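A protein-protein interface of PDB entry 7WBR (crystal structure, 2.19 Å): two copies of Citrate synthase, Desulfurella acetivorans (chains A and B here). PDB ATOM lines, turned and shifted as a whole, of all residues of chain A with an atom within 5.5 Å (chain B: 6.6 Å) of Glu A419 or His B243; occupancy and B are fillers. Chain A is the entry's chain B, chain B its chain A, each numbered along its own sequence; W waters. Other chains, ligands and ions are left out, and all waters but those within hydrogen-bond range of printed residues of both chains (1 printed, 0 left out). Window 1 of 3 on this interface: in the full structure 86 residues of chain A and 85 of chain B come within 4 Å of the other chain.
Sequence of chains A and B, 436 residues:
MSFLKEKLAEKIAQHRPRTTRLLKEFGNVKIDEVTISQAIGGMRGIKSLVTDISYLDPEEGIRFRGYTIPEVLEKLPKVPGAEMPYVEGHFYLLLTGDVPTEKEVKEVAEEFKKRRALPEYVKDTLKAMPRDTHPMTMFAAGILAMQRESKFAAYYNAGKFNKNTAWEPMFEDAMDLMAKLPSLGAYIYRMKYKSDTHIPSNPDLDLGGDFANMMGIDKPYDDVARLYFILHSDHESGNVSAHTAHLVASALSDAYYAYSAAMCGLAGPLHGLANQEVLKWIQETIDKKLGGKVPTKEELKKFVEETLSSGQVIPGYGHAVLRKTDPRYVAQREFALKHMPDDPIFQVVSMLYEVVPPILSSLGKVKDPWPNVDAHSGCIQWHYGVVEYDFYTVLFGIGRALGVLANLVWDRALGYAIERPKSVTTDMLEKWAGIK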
ATOM      1  N   MET A  43     -32.985 -14.629 -12.363  1.00  0.00           N
ATOM      2  CA  MET A  43     -33.715 -15.423 -13.337  1.00  0.00           C
ATOM      3  C   MET A  43     -35.254 -15.287 -13.317  1.00  0.00           C
ATOM      4  O   MET A  43     -35.931 -16.199 -13.767  1.00  0.00           O
ATOM      5  CB  MET A  43     -33.358 -16.905 -13.143  1.00  0.00           C
ATOM      6  CG  MET A  43     -31.860 -17.195 -12.954  1.00  0.00           C
ATOM      7  SD  MET A  43     -31.588 -18.966 -12.828  1.00  0.00           S
ATOM      8  CE  MET A  43     -29.816 -18.977 -12.767  1.00  0.00           C
ATOM      9  N   LEU A  49     -36.394 -24.800 -15.705  1.00  0.00           N
ATOM     10  CA  LEU A  49     -36.439 -26.015 -14.881  1.00  0.00           C
ATOM     11  C   LEU A  49     -37.610 -26.913 -15.261  1.00  0.00           C
ATOM     12  O   LEU A  49     -38.699 -26.448 -15.661  1.00  0.00           O
ATOM     13  CB  LEU A  49     -36.516 -25.625 -13.404  1.00  0.00           C
ATOM     14  CG  LEU A  49     -35.371 -24.816 -12.760  1.00  0.00           C
ATOM     15  CD1 LEU A  49     -35.754 -24.346 -11.374  1.00  0.00           C
ATOM     16  CD2 LEU A  49     -34.076 -25.595 -12.695  1.00  0.00           C
ATOM     17  N   HIS A 243     -35.066 -25.721  -5.473  1.00  0.00           N
ATOM     18  CA  HIS A 243     -34.052 -25.522  -6.493  1.00  0.00           C
ATOM     19  C   HIS A 243     -32.655 -25.837  -5.896  1.00  0.00           C
ATOM     20  O   HIS A 243     -31.863 -26.506  -6.521  1.00  0.00           O
ATOM     21  CB  HIS A 243     -34.147 -24.074  -6.969  1.00  0.00           C
ATOM     22  CG  HIS A 243     -33.179 -23.710  -8.036  1.00  0.00           C
ATOM     23  ND1 HIS A 243     -32.929 -22.396  -8.392  1.00  0.00           N
ATOM     24  CD2 HIS A 243     -32.406 -24.472  -8.831  1.00  0.00           C
ATOM     25  CE1 HIS A 243     -32.028 -22.371  -9.348  1.00  0.00           C
ATOM     26  NE2 HIS A 243     -31.697 -23.614  -9.637  1.00  0.00           N
ATOM     27  N   HIS A 246     -32.357 -29.492  -5.771  1.00  0.00           N
ATOM     28  CA  HIS A 246     -32.231 -29.950  -7.117  1.00  0.00           C
ATOM     29  C   HIS A 246     -30.808 -29.722  -7.659  1.00  0.00           C
ATOM     30  O   HIS A 246     -30.193 -30.626  -8.234  1.00  0.00           O
ATOM     31  CB  HIS A 246     -33.284 -29.233  -7.942  1.00  0.00           C
ATOM     32  CG  HIS A 246     -33.180 -29.499  -9.409  1.00  0.00           C
ATOM     33  ND1 HIS A 246     -33.527 -30.713  -9.971  1.00  0.00           N
ATOM     34  CD2 HIS A 246     -32.707 -28.730 -10.415  1.00  0.00           C
ATOM     35  CE1 HIS A 246     -33.299 -30.661 -11.279  1.00  0.00           C
ATOM     36  NE2 HIS A 246     -32.822 -29.465 -11.570  1.00  0.00           N
ATOM     37  N   LEU A 247     -30.303 -28.524  -7.450  1.00  0.00           N
ATOM     38  CA  LEU A 247     -28.946 -28.107  -7.894  1.00  0.00           C
ATOM     39  C   LEU A 247     -27.845 -28.987  -7.314  1.00  0.00           C
ATOM     40  O   LEU A 247     -27.009 -29.544  -8.054  1.00  0.00           O
ATOM     41  CB  LEU A 247     -28.708 -26.657  -7.477  1.00  0.00           C
ATOM     42  CG  LEU A 247     -27.363 -25.991  -7.781  1.00  0.00           C
ATOM     43  CD1 LEU A 247     -27.037 -26.129  -9.235  1.00  0.00           C
ATOM     44  CD2 LEU A 247     -27.429 -24.526  -7.377  1.00  0.00           C
ATOM     45  N   SER A 250     -28.049 -32.616  -8.492  1.00  0.00           N
ATOM     46  CA  SER A 250     -27.610 -32.724  -9.905  1.00  0.00           C
ATOM     47  C   SER A 250     -26.112 -32.946 -10.036  1.00  0.00           C
ATOM     48  O   SER A 250     -25.676 -33.387 -11.102  1.00  0.00           O
ATOM     49  CB  SER A 250     -28.010 -31.451 -10.700  1.00  0.00           C
ATOM     50  OG  SER A 250     -27.168 -30.342 -10.362  1.00  0.00           O
ATOM     51  N   ALA A 417     -29.194 -33.736 -15.907  1.00  0.00           N
ATOM     52  CA  ALA A 417     -27.730 -33.541 -15.903  1.00  0.00           C
ATOM     53  C   ALA A 417     -27.380 -32.458 -14.900  1.00  0.00           C
ATOM     54  O   ALA A 417     -28.237 -31.708 -14.441  1.00  0.00           O
ATOM     55  CB  ALA A 417     -27.246 -33.141 -17.340  1.00  0.00           C
ATOM     56  N   ILE A 418     -26.093 -32.346 -14.614  1.00  0.00           N
ATOM     57  CA  ILE A 418     -25.597 -31.338 -13.729  1.00  0.00           C
ATOM     58  C   ILE A 418     -26.149 -29.943 -14.107  1.00  0.00           C
ATOM     59  O   ILE A 418     -26.201 -29.608 -15.258  1.00  0.00           O
ATOM     60  CB  ILE A 418     -24.051 -31.405 -13.658  1.00  0.00           C
ATOM     61  CG1 ILE A 418     -23.524 -30.551 -12.481  1.00  0.00           C
ATOM     62  CG2 ILE A 418     -23.375 -31.067 -15.016  1.00  0.00           C
ATOM     63  CD1 ILE A 418     -22.025 -30.722 -12.240  1.00  0.00           C
ATOM     64  N   GLU A 419     -26.600 -29.148 -13.141  1.00  0.00           N
ATOM     65  CA  GLU A 419     -27.150 -27.869 -13.460  1.00  0.00           C
ATOM     66  C   GLU A 419     -25.964 -26.905 -13.489  1.00  0.00           C
ATOM     67  O   GLU A 419     -25.212 -26.798 -12.500  1.00  0.00           O
ATOM     68  CB  GLU A 419     -28.223 -27.432 -12.497  1.00  0.00           C
ATOM     69  CG  GLU A 419     -28.570 -25.937 -12.589  1.00  0.00           C
ATOM     70  CD  GLU A 419     -29.754 -25.565 -11.770  1.00  0.00           C
ATOM     71  OE1 GLU A 419     -30.702 -26.375 -11.706  1.00  0.00           O
ATOM     72  OE2 GLU A 419     -29.755 -24.445 -11.178  1.00  0.00           O
ATOM     73  N   ARG A 420     -25.766 -26.238 -14.642  1.00  0.00           N
ATOM     74  CA  ARG A 420     -24.533 -25.477 -14.896  1.00  0.00           C
ATOM     75  C   ARG A 420     -24.786 -24.385 -15.936  1.00  0.00           C
ATOM     76  O   ARG A 420     -24.441 -24.556 -17.112  1.00  0.00           O
ATOM     77  CB  ARG A 420     -23.425 -26.423 -15.392  1.00  0.00           C
ATOM     78  CG  ARG A 420     -22.014 -25.954 -15.152  1.00  0.00           C
ATOM     79  CD  ARG A 420     -21.778 -24.446 -15.364  1.00  0.00           C
ATOM     80  NE  ARG A 420     -20.429 -24.040 -14.969  1.00  0.00           N
ATOM     81  CZ  ARG A 420     -19.965 -22.781 -14.975  1.00  0.00           C
ATOM     82  NH1 ARG A 420     -20.741 -21.745 -15.379  1.00  0.00           N
ATOM     83  NH2 ARG A 420     -18.678 -22.568 -14.629  1.00  0.00           N
ATOM     84  N   PRO A 421     -25.426 -23.295 -15.519  1.00  0.00           N
ATOM     85  CA  PRO A 421     -25.711 -22.148 -16.386  1.00  0.00           C
ATOM     86  C   PRO A 421     -24.465 -21.278 -16.548  1.00  0.00           C
ATOM     87  O   PRO A 421     -23.467 -21.495 -15.860  1.00  0.00           O
ATOM     88  CB  PRO A 421     -26.779 -21.413 -15.616  1.00  0.00           C
ATOM     89  CG  PRO A 421     -26.483 -21.719 -14.182  1.00  0.00           C
ATOM     90  CD  PRO A 421     -25.963 -23.110 -14.158  1.00  0.00           C
ATOM     91  N   GLY B  41     -31.626 -30.466 -19.612  1.00  0.00           N
ATOM     92  CA  GLY B  41     -30.242 -30.778 -19.289  1.00  0.00           C
ATOM     93  C   GLY B  41     -29.552 -29.705 -18.465  1.00  0.00           C
ATOM     94  O   GLY B  41     -28.470 -29.261 -18.840  1.00  0.00           O
ATOM     95  N   GLY B  42     -30.168 -29.285 -17.359  1.00  0.00           N
ATOM     96  CA  GLY B  42     -29.465 -28.534 -16.343  1.00  0.00           C
ATOM     97  C   GLY B  42     -29.040 -27.135 -16.723  1.00  0.00           C
ATOM     98  O   GLY B  42     -27.907 -26.701 -16.391  1.00  0.00           O
ATOM     99  N   MET B  43     -29.975 -26.432 -17.390  1.00  0.00           N
ATOM    100  CA  MET B  43     -29.799 -25.074 -17.907  1.00  0.00           C
ATOM    101  C   MET B  43     -28.471 -24.845 -18.667  1.00  0.00           C
ATOM    102  O   MET B  43     -27.957 -23.740 -18.626  1.00  0.00           O
ATOM    103  CB  MET B  43     -29.837 -24.037 -16.775  1.00  0.00           C
ATOM    104  CG  MET B  43     -30.864 -24.135 -15.684  1.00  0.00           C
ATOM    105  SD  MET B  43     -30.448 -22.811 -14.526  1.00  0.00           S
ATOM    106  CE  MET B  43     -32.034 -22.687 -13.734  1.00  0.00           C
ATOM    107  N   ARG B  44     -27.939 -25.886 -19.306  1.00  0.00           N
ATOM    108  CA  ARG B  44     -26.619 -25.932 -19.925  1.00  0.00           C
ATOM    109  C   ARG B  44     -26.358 -24.707 -20.795  1.00  0.00           C
ATOM    110  O   ARG B  44     -27.031 -24.509 -21.822  1.00  0.00           O
ATOM    111  CB  ARG B  44     -26.517 -27.194 -20.809  1.00  0.00           C
ATOM    112  CG  ARG B  44     -25.241 -27.315 -21.659  1.00  0.00           C
ATOM    113  CD  ARG B  44     -25.054 -28.685 -22.339  1.00  0.00           C
ATOM    114  NE  ARG B  44     -26.302 -29.321 -22.823  1.00  0.00           N
ATOM    115  CZ  ARG B  44     -26.927 -30.377 -22.268  1.00  0.00           C
ATOM    116  NH1 ARG B  44     -26.466 -31.005 -21.169  1.00  0.00           N
ATOM    117  NH2 ARG B  44     -28.054 -30.819 -22.827  1.00  0.00           N
ATOM    118  N   LEU B  49     -26.908 -15.600 -15.251  1.00  0.00           N
ATOM    119  CA  LEU B  49     -26.272 -15.169 -13.995  1.00  0.00           C
ATOM    120  C   LEU B  49     -25.258 -14.084 -14.283  1.00  0.00           C
ATOM    121  O   LEU B  49     -24.639 -14.086 -15.319  1.00  0.00           O
ATOM    122  CB  LEU B  49     -25.559 -16.366 -13.249  1.00  0.00           C
ATOM    123  CG  LEU B  49     -26.419 -17.452 -12.577  1.00  0.00           C
ATOM    124  CD1 LEU B  49     -25.576 -18.694 -12.366  1.00  0.00           C
ATOM    125  CD2 LEU B  49     -27.037 -17.005 -11.258  1.00  0.00           C
ATOM    126  N   GLU B 236     -16.165 -18.409 -12.120  1.00  0.00           N
ATOM    127  CA  GLU B 236     -17.388 -17.663 -12.202  1.00  0.00           C
ATOM    128  C   GLU B 236     -18.504 -18.234 -11.251  1.00  0.00           C
ATOM    129  O   GLU B 236     -18.200 -18.967 -10.294  1.00  0.00           O
ATOM    130  CB  GLU B 236     -17.778 -17.473 -13.696  1.00  0.00           C
ATOM    131  CG  GLU B 236     -18.315 -18.674 -14.412  1.00  0.00           C
ATOM    132  CD  GLU B 236     -18.817 -18.390 -15.829  1.00  0.00           C
ATOM    133  OE1 GLU B 236     -18.172 -17.549 -16.537  1.00  0.00           O
ATOM    134  OE2 GLU B 236     -19.844 -19.061 -16.222  1.00  0.00           O
ATOM    135  N   SER B 237     -19.765 -17.883 -11.489  1.00  0.00           N
ATOM    136  CA  SER B 237     -20.818 -18.121 -10.516  1.00  0.00           C
ATOM    137  C   SER B 237     -21.720 -19.271 -10.885  1.00  0.00           C
ATOM    138  O   SER B 237     -22.586 -19.619 -10.089  1.00  0.00           O
ATOM    139  CB  SER B 237     -21.677 -16.862 -10.327  1.00  0.00           C
ATOM    140  OG  SER B 237     -22.571 -16.664 -11.403  1.00  0.00           O
ATOM    141  N   GLY B 238     -21.565 -19.813 -12.100  1.00  0.00           N
ATOM    142  CA  GLY B 238     -22.459 -20.838 -12.607  1.00  0.00           C
ATOM    143  C   GLY B 238     -22.080 -22.267 -12.288  1.00  0.00           C
ATOM    144  O   GLY B 238     -22.871 -23.143 -12.472  1.00  0.00           O
ATOM    145  N   ASN B 239     -20.878 -22.499 -11.791  1.00  0.00           N
ATOM    146  CA  ASN B 239     -20.544 -23.803 -11.209  1.00  0.00           C
ATOM    147  C   ASN B 239     -21.415 -24.133  -9.987  1.00  0.00           C
ATOM    148  O   ASN B 239     -22.010 -23.241  -9.355  1.00  0.00           O
ATOM    149  CB  ASN B 239     -19.050 -23.885 -10.890  1.00  0.00           C
ATOM    150  CG  ASN B 239     -18.638 -23.024  -9.715  1.00  0.00           C
ATOM    151  OD1 ASN B 239     -18.815 -23.419  -8.574  1.00  0.00           O
ATOM    152  ND2 ASN B 239     -17.970 -21.886  -9.992  1.00  0.00           N
ATOM    153  N   VAL B 240     -21.544 -25.414  -9.699  1.00  0.00           N
ATOM    154  CA  VAL B 240     -22.596 -25.858  -8.766  1.00  0.00           C
ATOM    155  C   VAL B 240     -22.431 -25.210  -7.402  1.00  0.00           C
ATOM    156  O   VAL B 240     -23.370 -24.598  -6.877  1.00  0.00           O
ATOM    157  CB  VAL B 240     -22.664 -27.353  -8.688  1.00  0.00           C
ATOM    158  CG1 VAL B 240     -23.438 -27.814  -7.467  1.00  0.00           C
ATOM    159  CG2 VAL B 240     -23.306 -27.889  -9.952  1.00  0.00           C
ATOM    160  N   SER B 241     -21.213 -25.221  -6.902  1.00  0.00           N
ATOM    161  CA  SER B 241     -20.953 -24.756  -5.549  1.00  0.00           C
ATOM    162  C   SER B 241     -21.119 -23.229  -5.425  1.00  0.00           C
ATOM    163  O   SER B 241     -21.834 -22.749  -4.536  1.00  0.00           O
ATOM    164  CB  SER B 241     -19.593 -25.191  -5.074  1.00  0.00           C
ATOM    165  OG  SER B 241     -18.553 -24.622  -5.841  1.00  0.00           O
ATOM    166  N   ALA B 242     -20.517 -22.478  -6.337  1.00  0.00           N
ATOM    167  CA  ALA B 242     -20.686 -21.026  -6.332  1.00  0.00           C
ATOM    168  C   ALA B 242     -22.148 -20.583  -6.537  1.00  0.00           C
ATOM    169  O   ALA B 242     -22.619 -19.624  -5.914  1.00  0.00           O
ATOM    170  CB  ALA B 242     -19.784 -20.392  -7.377  1.00  0.00           C
ATOM    171  N   HIS B 243     -22.814 -21.239  -7.459  1.00  0.00           N
ATOM    172  CA  HIS B 243     -24.236 -21.025  -7.749  1.00  0.00           C
ATOM    173  C   HIS B 243     -25.106 -21.378  -6.564  1.00  0.00           C
ATOM    174  O   HIS B 243     -26.015 -20.655  -6.239  1.00  0.00           O
ATOM    175  CB  HIS B 243     -24.606 -21.921  -8.917  1.00  0.00           C
ATOM    176  CG  HIS B 243     -25.980 -21.729  -9.418  1.00  0.00           C
ATOM    177  ND1 HIS B 243     -26.547 -22.589 -10.329  1.00  0.00           N
ATOM    178  CD2 HIS B 243     -26.903 -20.780  -9.166  1.00  0.00           C
ATOM    179  CE1 HIS B 243     -27.774 -22.186 -10.594  1.00  0.00           C
ATOM    180  NE2 HIS B 243     -28.021 -21.104  -9.897  1.00  0.00           N
ATOM    181  N   THR B 244     -24.795 -22.486  -5.883  1.00  0.00           N
ATOM    182  CA  THR B 244     -25.539 -22.853  -4.672  1.00  0.00           C
ATOM    183  C   THR B 244     -25.396 -21.802  -3.622  1.00  0.00           C
ATOM    184  O   THR B 244     -26.396 -21.386  -3.022  1.00  0.00           O
ATOM    185  CB  THR B 244     -25.103 -24.250  -4.149  1.00  0.00           C
ATOM    186  OG1 THR B 244     -25.394 -25.231  -5.162  1.00  0.00           O
ATOM    187  CG2 THR B 244     -25.820 -24.603  -2.841  1.00  0.00           C
ATOM    188  N   ALA B 245     -24.166 -21.322  -3.380  1.00  0.00           N
ATOM    189  CA  ALA B 245     -24.022 -20.286  -2.365  1.00  0.00           C
ATOM    190  C   ALA B 245     -24.817 -19.041  -2.801  1.00  0.00           C
ATOM    191  O   ALA B 245     -25.495 -18.378  -1.991  1.00  0.00           O
ATOM    192  CB  ALA B 245     -22.560 -19.925  -2.169  1.00  0.00           C
ATOM    193  N   HIS B 246     -24.718 -18.714  -4.098  1.00  0.00           N
ATOM    194  CA  HIS B 246     -25.345 -17.488  -4.651  1.00  0.00           C
ATOM    195  C   HIS B 246     -26.839 -17.559  -4.460  1.00  0.00           C
ATOM    196  O   HIS B 246     -27.476 -16.660  -3.890  1.00  0.00           O
ATOM    197  CB  HIS B 246     -24.982 -17.351  -6.144  1.00  0.00           C
ATOM    198  CG  HIS B 246     -25.797 -16.332  -6.862  1.00  0.00           C
ATOM    199  ND1 HIS B 246     -25.699 -14.980  -6.599  1.00  0.00           N
ATOM    200  CD2 HIS B 246     -26.783 -16.477  -7.776  1.00  0.00           C
ATOM    201  CE1 HIS B 246     -26.562 -14.334  -7.369  1.00  0.00           C
ATOM    202  NE2 HIS B 246     -27.224 -15.221  -8.101  1.00  0.00           N
ATOM    203  N   LEU B 247     -27.381 -18.694  -4.884  1.00  0.00           N
ATOM    204  CA  LEU B 247     -28.815 -18.996  -4.720  1.00  0.00           C
ATOM    205  C   LEU B 247     -29.328 -18.891  -3.291  1.00  0.00           C
ATOM    206  O   LEU B 247     -30.329 -18.188  -2.953  1.00  0.00           O
ATOM    207  CB  LEU B 247     -29.028 -20.403  -5.298  1.00  0.00           C
ATOM    208  CG  LEU B 247     -30.387 -21.103  -5.143  1.00  0.00           C
ATOM    209  CD1 LEU B 247     -31.560 -20.332  -5.711  1.00  0.00           C
ATOM    210  CD2 LEU B 247     -30.294 -22.452  -5.798  1.00  0.00           C
ATOM    211  N   VAL B 248     -28.650 -19.585  -2.398  1.00  0.00           N
ATOM    212  CA  VAL B 248     -29.074 -19.548  -0.965  1.00  0.00           C
ATOM    213  C   VAL B 248     -28.990 -18.158  -0.408  1.00  0.00           C
ATOM    214  O   VAL B 248     -29.957 -17.658   0.203  1.00  0.00           O
ATOM    215  CB  VAL B 248     -28.307 -20.644  -0.117  1.00  0.00           C
ATOM    216  CG1 VAL B 248     -28.528 -20.506   1.373  1.00  0.00           C
ATOM    217  CG2 VAL B 248     -28.718 -22.037  -0.608  1.00  0.00           C
ATOM    218  N   VAL B 404     -16.314 -17.214  -3.828  1.00  0.00           N
ATOM    219  CA  VAL B 404     -17.708 -17.235  -3.465  1.00  0.00           C
ATOM    220  C   VAL B 404     -18.094 -16.185  -2.468  1.00  0.00           C
ATOM    221  O   VAL B 404     -19.121 -15.474  -2.670  1.00  0.00           O
ATOM    222  CB  VAL B 404     -18.159 -18.620  -2.974  1.00  0.00           C
ATOM    223  CG1 VAL B 404     -19.639 -18.617  -2.583  1.00  0.00           C
ATOM    224  CG2 VAL B 404     -17.958 -19.591  -4.097  1.00  0.00           C
ATOM    225  N   GLU B 419     -33.242 -15.463  -6.299  1.00  0.00           N
ATOM    226  CA  GLU B 419     -33.223 -16.258  -7.506  1.00  0.00           C
ATOM    227  C   GLU B 419     -34.361 -17.287  -7.488  1.00  0.00           C
ATOM    228  O   GLU B 419     -34.498 -18.099  -6.560  1.00  0.00           O
ATOM    229  CB  GLU B 419     -31.882 -16.948  -7.687  1.00  0.00           C
ATOM    230  CG  GLU B 419     -31.816 -17.894  -8.873  1.00  0.00           C
ATOM    231  CD  GLU B 419     -30.455 -18.489  -9.062  1.00  0.00           C
ATOM    232  OE1 GLU B 419     -29.470 -17.788  -8.898  1.00  0.00           O
ATOM    233  OE2 GLU B 419     -30.333 -19.656  -9.390  1.00  0.00           O
ATOM    234  N   PRO B 421     -36.322 -18.903 -10.818  1.00  0.00           N
ATOM    235  CA  PRO B 421     -36.823 -19.178 -12.157  1.00  0.00           C
ATOM    236  C   PRO B 421     -38.131 -19.917 -12.094  1.00  0.00           C
ATOM    237  O   PRO B 421     -38.589 -20.251 -10.991  1.00  0.00           O
ATOM    238  CB  PRO B 421     -35.746 -20.058 -12.743  1.00  0.00           C
ATOM    239  CG  PRO B 421     -35.235 -20.831 -11.576  1.00  0.00           C
ATOM    240  CD  PRO B 421     -35.392 -19.953 -10.358  1.00  0.00           C
HETATM  241  O   HOH W   1     -24.776 -24.571 -11.244  1.00  0.00           O
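The backbone carbonyl oxygen (O) of Gly B42 is in hydrogen-bond range of the backbone NH (N) of Arg A420 (2.8 Å).
OE2 of Glu B236 lies within salt-bridge range of NH1 of Arg A420, at 3.0 Å.
The side-chain carboxylate of Glu B419 lies close to the side-chain sulfur of Met A43 (3.7 Å).
The side-chain carboxylate of Glu A419 lies close to the side-chain sulfur of Met B43, 3.8 Å away.
The backbone carbonyl oxygen (O) of Glu B236 sits at hydrogen-bond distance from the side-chain amide nitrogen (ND2) of Asn B239, at 2.9 Å.
OG of Ser B241 lies within hydrogen-bond range of OD1 of Asn B239 (3.0 Å).
O of Val B240 lies within hydrogen-bond range of OG1 of Thr B244 (2.7 Å).
A ring nitrogen (NE2) of His B243 sits at hydrogen-bond distance from the side-chain carboxylate (OE2) of Glu B419, at 2.8 Å.
The side-chain carboxylate (OE2) of Glu A419 lies within hydrogen-bond range of a ring nitrogen (NE2) of His A243 (2.6 Å).
OG of Ser A250 lies within hydrogen-bond range of N of Glu A419 (3.1 Å).
Met B43 touches Met A43.
CE of Met B43 touches CD2 of Leu A49 (3.7 Å).
CA of Gly B42 touches O of Ala A417, at 3.9 Å.
Glu A419 touches Gly B42 (CA to O, 3.2 Å).
Met B43 touches Arg A420.
O of Arg A420 touches CA of Arg B44, at 3.8 Å.
CD of Arg A420 touches O of Gly B238, at 3.4 Å.
N of Asn B239 touches CZ of Arg A420, 3.3 Å away.
CG of Pro A421 touches CD1 of Leu B49, 3.6 Å away.
Pro A421 touches His B243 (CG to CE1, 3.8 Å).
Of the printed residues of chain B, His A243 touches Leu B247 (3.6 Å), Glu B419 (3.2 Å) and Pro B421 (3.99 Å).
Ser A250 touches none of the printed residues of chain B.
Of the printed residues of chain B, Pro A421 touches Met B43, Leu B49, Gly B238 and His B243.
Of the printed residues of chain A, Arg B44 touches Arg A420 (3.8 Å).
Of the printed residues of chain A, Leu B247 touches His A243 (3.6 Å) and Leu A247 (3.9 Å).
Val B248 touches none of the printed residues of chain A.
The nearest printed residue of chain A that does not touch His B243 is His A243 (4.2 Å).
Of the 11 printed residues of chain A, 9 touch a printed residue of chain B.
Hydrophobic or aromatic side chains of chain A that line the printed part of chain B: Met A43, Leu A49, His A243, Leu A247, Ile A418 and Pro A421.
Of the 21 printed residues of chain B, 13 touch a printed residue of chain A.
Hydrophobic or aromatic side chains of chain B within 4 Å of the printed part of chain A: Met B43, Leu B49, Val B240, His B243, Leu B247 and Pro B421.
Among the printed residues, 30 pairs touch across the chains.
Among the printed residues, Asp or Glu carboxylates within 4 Å of a Lys or Arg side-chain nitrogen of the other chain: Arg A420 with Glu B236 (3.0 Å).
Met A43 touches His B243, but with the chains exchanged His A243 does not touch Met B43 (4.2 Å).
Met A43 touches Pro B421, and with the chains exchanged Pro A421 touches Met B43.
His A243 touches Leu B247, and with the chains exchanged Leu A247 touches His B243.
His A243 touches Pro B421, and with the chains exchanged Pro A421 touches His B243.
Of the 30 pairs that touch across the chains among the printed residues, 16 have their exchanged pair printed and touching as well.
Water W1 lies within hydrogen-bond range of O of Glu A419 (2.6 Å), O of Gly B238 (2.7 Å) and ND1 of His B243 (2.8 Å).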
